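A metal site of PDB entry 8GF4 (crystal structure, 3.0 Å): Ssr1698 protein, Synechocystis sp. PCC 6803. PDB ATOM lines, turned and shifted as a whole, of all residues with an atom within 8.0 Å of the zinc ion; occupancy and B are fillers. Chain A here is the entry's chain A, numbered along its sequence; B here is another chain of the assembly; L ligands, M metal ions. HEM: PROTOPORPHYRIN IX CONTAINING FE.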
ATOM      1  N   SER A  75     -24.501 -11.212   7.293  1.00  0.00           N
ATOM      2  CA  SER A  75     -24.359 -12.614   7.776  1.00  0.00           C
ATOM      3  C   SER A  75     -22.917 -12.905   8.211  1.00  0.00           C
ATOM      4  O   SER A  75     -22.746 -13.586   9.235  1.00  0.00           O
ATOM      5  CB  SER A  75     -24.788 -13.590   6.720  1.00  0.00           C
ATOM      6  OG  SER A  75     -26.101 -13.300   6.264  1.00  0.00           O
ATOM      7  N   GLU A  76     -21.933 -12.439   7.441  1.00  0.00           N
ATOM      8  CA  GLU A  76     -20.474 -12.572   7.738  1.00  0.00           C
ATOM      9  C   GLU A  76     -20.188 -12.015   9.152  1.00  0.00           C
ATOM     10  O   GLU A  76     -19.487 -12.686   9.924  1.00  0.00           O
ATOM     11  CB  GLU A  76     -19.628 -11.873   6.666  1.00  0.00           C
ATOM     12  CG  GLU A  76     -18.154 -11.837   6.997  1.00  0.00           C
ATOM     13  CD  GLU A  76     -17.505 -13.205   7.194  1.00  0.00           C
ATOM     14  OE1 GLU A  76     -18.086 -14.213   6.742  1.00  0.00           O
ATOM     15  OE2 GLU A  76     -16.403 -13.271   7.792  1.00  0.00           O
ATOM     16  N   ASP A  77     -20.740 -10.853   9.493  1.00  0.00           N
ATOM     17  CA  ASP A  77     -20.760 -10.326  10.881  1.00  0.00           C
ATOM     18  C   ASP A  77     -20.976 -11.502  11.843  1.00  0.00           C
ATOM     19  O   ASP A  77     -20.187 -11.612  12.785  1.00  0.00           O
ATOM     20  CB  ASP A  77     -21.801  -9.206  11.045  1.00  0.00           C
ATOM     21  CG  ASP A  77     -21.356  -7.795  10.664  1.00  0.00           C
ATOM     22  OD1 ASP A  77     -20.592  -7.658   9.673  1.00  0.00           O
ATOM     23  OD2 ASP A  77     -21.782  -6.832  11.356  1.00  0.00           O
ATOM     24  N   ALA A  78     -21.957 -12.383  11.587  1.00  0.00           N
ATOM     25  CA  ALA A  78     -22.322 -13.555  12.433  1.00  0.00           C
ATOM     26  C   ALA A  78     -21.181 -14.581  12.404  1.00  0.00           C
ATOM     27  O   ALA A  78     -20.821 -15.089  13.485  1.00  0.00           O
ATOM     28  CB  ALA A  78     -23.620 -14.197  11.987  1.00  0.00           C
ATOM     29  N   HIS A  79     -20.640 -14.879  11.232  1.00  0.00           N
ATOM     30  CA  HIS A  79     -19.447 -15.750  11.089  1.00  0.00           C
ATOM     31  C   HIS A  79     -18.332 -15.187  11.959  1.00  0.00           C
ATOM     32  O   HIS A  79     -17.805 -15.934  12.814  1.00  0.00           O
ATOM     33  CB  HIS A  79     -19.056 -15.835   9.624  1.00  0.00           C
ATOM     34  CG  HIS A  79     -18.259 -17.041   9.307  1.00  0.00           C
ATOM     35  ND1 HIS A  79     -17.182 -17.001   8.460  1.00  0.00           N
ATOM     36  CD2 HIS A  79     -18.371 -18.305   9.752  1.00  0.00           C
ATOM     37  CE1 HIS A  79     -16.656 -18.214   8.368  1.00  0.00           C
ATOM     38  NE2 HIS A  79     -17.372 -19.033   9.154  1.00  0.00           N
ATOM     39  N   GLN A  80     -18.060 -13.890  11.809  1.00  0.00           N
ATOM     40  CA  GLN A  80     -16.920 -13.178  12.445  1.00  0.00           C
ATOM     41  C   GLN A  80     -17.091 -13.194  13.967  1.00  0.00           C
ATOM     42  O   GLN A  80     -16.057 -13.279  14.660  1.00  0.00           O
ATOM     43  CB  GLN A  80     -16.792 -11.730  11.959  1.00  0.00           C
ATOM     44  CG  GLN A  80     -16.548 -11.594  10.455  1.00  0.00           C
ATOM     45  CD  GLN A  80     -15.110 -11.733   9.990  1.00  0.00           C
ATOM     46  OE1 GLN A  80     -14.281 -12.460  10.555  1.00  0.00           O
ATOM     47  NE2 GLN A  80     -14.806 -11.008   8.911  1.00  0.00           N
ATOM     48  N   ILE A  83     -16.601 -16.840  15.257  1.00  0.00           N
ATOM     49  CA  ILE A  83     -15.137 -17.124  15.322  1.00  0.00           C
ATOM     50  C   ILE A  83     -14.565 -16.335  16.515  1.00  0.00           C
ATOM     51  O   ILE A  83     -13.817 -16.917  17.327  1.00  0.00           O
ATOM     52  CB  ILE A  83     -14.390 -16.888  13.983  1.00  0.00           C
ATOM     53  CG1 ILE A  83     -13.783 -15.486  13.851  1.00  0.00           C
ATOM     54  CG2 ILE A  83     -15.276 -17.235  12.789  1.00  0.00           C
ATOM     55  CD1 ILE A  83     -12.339 -15.342  14.333  1.00  0.00           C
ATOM     56  N   HIS B  16     -15.046 -16.885  -0.593  1.00  0.00           N
ATOM     57  CA  HIS B  16     -15.378 -16.459   0.799  1.00  0.00           C
ATOM     58  C   HIS B  16     -14.115 -16.271   1.616  1.00  0.00           C
ATOM     59  O   HIS B  16     -13.980 -15.221   2.285  1.00  0.00           O
ATOM     60  CB  HIS B  16     -16.254 -17.453   1.539  1.00  0.00           C
ATOM     61  CG  HIS B  16     -16.735 -16.919   2.845  1.00  0.00           C
ATOM     62  ND1 HIS B  16     -17.596 -15.844   2.914  1.00  0.00           N
ATOM     63  CD2 HIS B  16     -16.469 -17.292   4.115  1.00  0.00           C
ATOM     64  CE1 HIS B  16     -17.878 -15.593   4.175  1.00  0.00           C
ATOM     65  NE2 HIS B  16     -17.196 -16.467   4.940  1.00  0.00           N
ATOM     66  N   MET B  17     -13.247 -17.278   1.562  1.00  0.00           N
ATOM     67  CA  MET B  17     -11.918 -17.242   2.206  1.00  0.00           C
ATOM     68  C   MET B  17     -11.177 -15.997   1.734  1.00  0.00           C
ATOM     69  O   MET B  17     -10.606 -15.284   2.601  1.00  0.00           O
ATOM     70  CB  MET B  17     -11.110 -18.501   1.854  1.00  0.00           C
ATOM     71  CG  MET B  17     -11.612 -19.754   2.581  1.00  0.00           C
ATOM     72  SD  MET B  17     -11.719 -19.624   4.408  1.00  0.00           S
ATOM     73  CE  MET B  17     -10.005 -19.284   4.787  1.00  0.00           C
ATOM     74  N   GLU B  19     -12.285 -13.074   0.258  1.00  0.00           N
ATOM     75  CA  GLU B  19     -12.878 -11.739   0.542  1.00  0.00           C
ATOM     76  C   GLU B  19     -13.024 -11.497   2.053  1.00  0.00           C
ATOM     77  O   GLU B  19     -13.019 -10.308   2.435  1.00  0.00           O
ATOM     78  CB  GLU B  19     -14.189 -11.513  -0.234  1.00  0.00           C
ATOM     79  CG  GLU B  19     -15.306 -12.468   0.087  1.00  0.00           C
ATOM     80  CD  GLU B  19     -16.565 -12.286  -0.762  1.00  0.00           C
ATOM     81  OE1 GLU B  19     -17.589 -11.845  -0.204  1.00  0.00           O
ATOM     82  OE2 GLU B  19     -16.529 -12.616  -1.957  1.00  0.00           O
ATOM     83  N   ASP B  20     -13.094 -12.540   2.891  1.00  0.00           N
ATOM     84  CA  ASP B  20     -13.575 -12.395   4.293  1.00  0.00           C
ATOM     85  C   ASP B  20     -12.631 -13.048   5.347  1.00  0.00           C
ATOM     86  O   ASP B  20     -12.984 -12.972   6.549  1.00  0.00           O
ATOM     87  CB  ASP B  20     -15.034 -12.857   4.356  1.00  0.00           C
ATOM     88  CG  ASP B  20     -16.008 -11.750   3.967  1.00  0.00           C
ATOM     89  OD1 ASP B  20     -15.728 -10.578   4.303  1.00  0.00           O
ATOM     90  OD2 ASP B  20     -17.052 -12.058   3.328  1.00  0.00           O
ATOM     91  N   HIS B  21     -11.479 -13.615   4.965  1.00  0.00           N
ATOM     92  CA  HIS B  21     -10.584 -14.327   5.922  1.00  0.00           C
ATOM     93  C   HIS B  21      -9.158 -14.496   5.388  1.00  0.00           C
ATOM     94  O   HIS B  21      -8.597 -15.583   5.554  1.00  0.00           O
ATOM     95  CB  HIS B  21     -11.104 -15.729   6.242  1.00  0.00           C
ATOM     96  CG  HIS B  21     -12.412 -15.759   6.946  1.00  0.00           C
ATOM     97  ND1 HIS B  21     -12.499 -15.587   8.300  1.00  0.00           N
ATOM     98  CD2 HIS B  21     -13.653 -15.972   6.471  1.00  0.00           C
ATOM     99  CE1 HIS B  21     -13.774 -15.679   8.650  1.00  0.00           C
ATOM    100  NE2 HIS B  21     -14.509 -15.910   7.528  1.00  0.00           N
ATOM    101  N   HIS B  79     -14.268 -27.157   6.058  1.00  0.00           N
ATOM    102  CA  HIS B  79     -14.413 -26.145   7.136  1.00  0.00           C
ATOM    103  C   HIS B  79     -13.505 -26.527   8.328  1.00  0.00           C
ATOM    104  O   HIS B  79     -12.636 -25.713   8.696  1.00  0.00           O
ATOM    105  CB  HIS B  79     -15.885 -26.097   7.517  1.00  0.00           C
ATOM    106  CG  HIS B  79     -16.280 -24.918   8.298  1.00  0.00           C
ATOM    107  ND1 HIS B  79     -17.330 -24.956   9.181  1.00  0.00           N
ATOM    108  CD2 HIS B  79     -15.799 -23.663   8.326  1.00  0.00           C
ATOM    109  CE1 HIS B  79     -17.487 -23.773   9.734  1.00  0.00           C
ATOM    110  NE2 HIS B  79     -16.558 -22.961   9.231  1.00  0.00           N
HETATM  111  CHA HEM L   1     -14.325 -20.561  11.921  1.00  0.00           C
HETATM  112  CHB HEM L   1     -14.247 -20.608   7.037  1.00  0.00           C
HETATM  113  CHC HEM L   1     -19.093 -21.141   6.923  1.00  0.00           C
HETATM  114  CHD HEM L   1     -19.193 -21.261  11.829  1.00  0.00           C
HETATM  115  C1A HEM L   1     -13.870 -20.542  10.545  1.00  0.00           C
HETATM  116  C2A HEM L   1     -12.464 -20.353  10.225  1.00  0.00           C
HETATM  117  C3A HEM L   1     -12.462 -20.338   8.779  1.00  0.00           C
HETATM  118  C4A HEM L   1     -13.864 -20.547   8.447  1.00  0.00           C
HETATM  119  CMA HEM L   1     -11.321 -20.193   7.844  1.00  0.00           C
HETATM  120  CAA HEM L   1     -11.287 -20.131  11.098  1.00  0.00           C
HETATM  121  CBA HEM L   1     -11.385 -18.676  11.506  1.00  0.00           C
HETATM  122  CGA HEM L   1     -10.090 -18.111  12.041  1.00  0.00           C
HETATM  123  O1A HEM L   1      -9.856 -16.897  11.810  1.00  0.00           O
HETATM  124  O2A HEM L   1      -9.308 -18.820  12.729  1.00  0.00           O
HETATM  125  C1B HEM L   1     -15.604 -20.746   6.520  1.00  0.00           C
HETATM  126  C2B HEM L   1     -15.869 -20.759   5.063  1.00  0.00           C
HETATM  127  C3B HEM L   1     -17.313 -20.922   5.047  1.00  0.00           C
HETATM  128  C4B HEM L   1     -17.688 -20.990   6.475  1.00  0.00           C
HETATM  129  CMB HEM L   1     -14.879 -20.613   3.950  1.00  0.00           C
HETATM  130  CAB HEM L   1     -18.234 -20.979   3.872  1.00  0.00           C
HETATM  131  CBB HEM L   1     -17.725 -21.977   2.848  1.00  0.00           C
HETATM  132  C1C HEM L   1     -19.589 -21.208   8.316  1.00  0.00           C
HETATM  133  C2C HEM L   1     -21.057 -21.303   8.613  1.00  0.00           C
HETATM  134  C3C HEM L   1     -21.011 -21.360  10.080  1.00  0.00           C
HETATM  135  C4C HEM L   1     -19.617 -21.269  10.444  1.00  0.00           C
HETATM  136  CMC HEM L   1     -22.162 -21.446   7.608  1.00  0.00           C
HETATM  137  CAC HEM L   1     -22.074 -21.477  11.072  1.00  0.00           C
HETATM  138  CBC HEM L   1     -23.337 -21.490  10.728  1.00  0.00           C
HETATM  139  C1D HEM L   1     -17.812 -21.083  12.258  1.00  0.00           C
HETATM  140  C2D HEM L   1     -17.504 -21.073  13.683  1.00  0.00           C
HETATM  141  C3D HEM L   1     -16.086 -20.803  13.755  1.00  0.00           C
HETATM  142  C4D HEM L   1     -15.708 -20.731  12.319  1.00  0.00           C
HETATM  143  CMD HEM L   1     -18.454 -21.201  14.796  1.00  0.00           C
HETATM  144  CAD HEM L   1     -15.282 -20.748  15.016  1.00  0.00           C
HETATM  145  CBD HEM L   1     -15.045 -22.231  15.256  1.00  0.00           C
HETATM  146  CGD HEM L   1     -14.062 -22.625  16.316  1.00  0.00           C
HETATM  147  O1D HEM L   1     -13.499 -21.847  17.119  1.00  0.00           O
HETATM  148  O2D HEM L   1     -13.862 -23.832  16.303  1.00  0.00           O
HETATM  149  NA  HEM L   1     -14.681 -20.667   9.485  1.00  0.00           N
HETATM  150  NB  HEM L   1     -16.658 -20.897   7.319  1.00  0.00           N
HETATM  151  NC  HEM L   1     -18.787 -21.175   9.398  1.00  0.00           N
HETATM  152  ND  HEM L   1     -16.741 -20.894  11.474  1.00  0.00           N
HETATM  153 FE   HEM L   1     -16.731 -20.951   9.397  1.00  0.00          FE
HETATM  154 ZN    ZN M   1     -16.442 -15.790   6.921  1.00  0.00          ZN
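A ring nitrogen (NE2) of His 79 of chain B is bound to an iron atom (FE) of the ligand (2.0 Å). A ring nitrogen (NE2) of His 79 of chain A binds an iron atom (FE) of the ligand, 2.0 Å away.
OE2 of Glu 76 sits close to NE2 of Gln 80 (3.0 Å).
NE2 of His 21 of chain B is bound to the zinc ion. The zinc ion is bound by a ring nitrogen (ND1) of His 79 of chain A (2.1 Å). NE2 of His 16 of chain B is bound to the zinc ion, 2.2 Å away. The zinc ion is bound by the side-chain carboxylate (OE1) of Glu 76 (2.3 Å). The zinc ion has four donor atoms within binding distance. Slightly farther from the zinc ion lies the side-chain carboxylate (OE2) of Glu 76 (2.7 Å).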
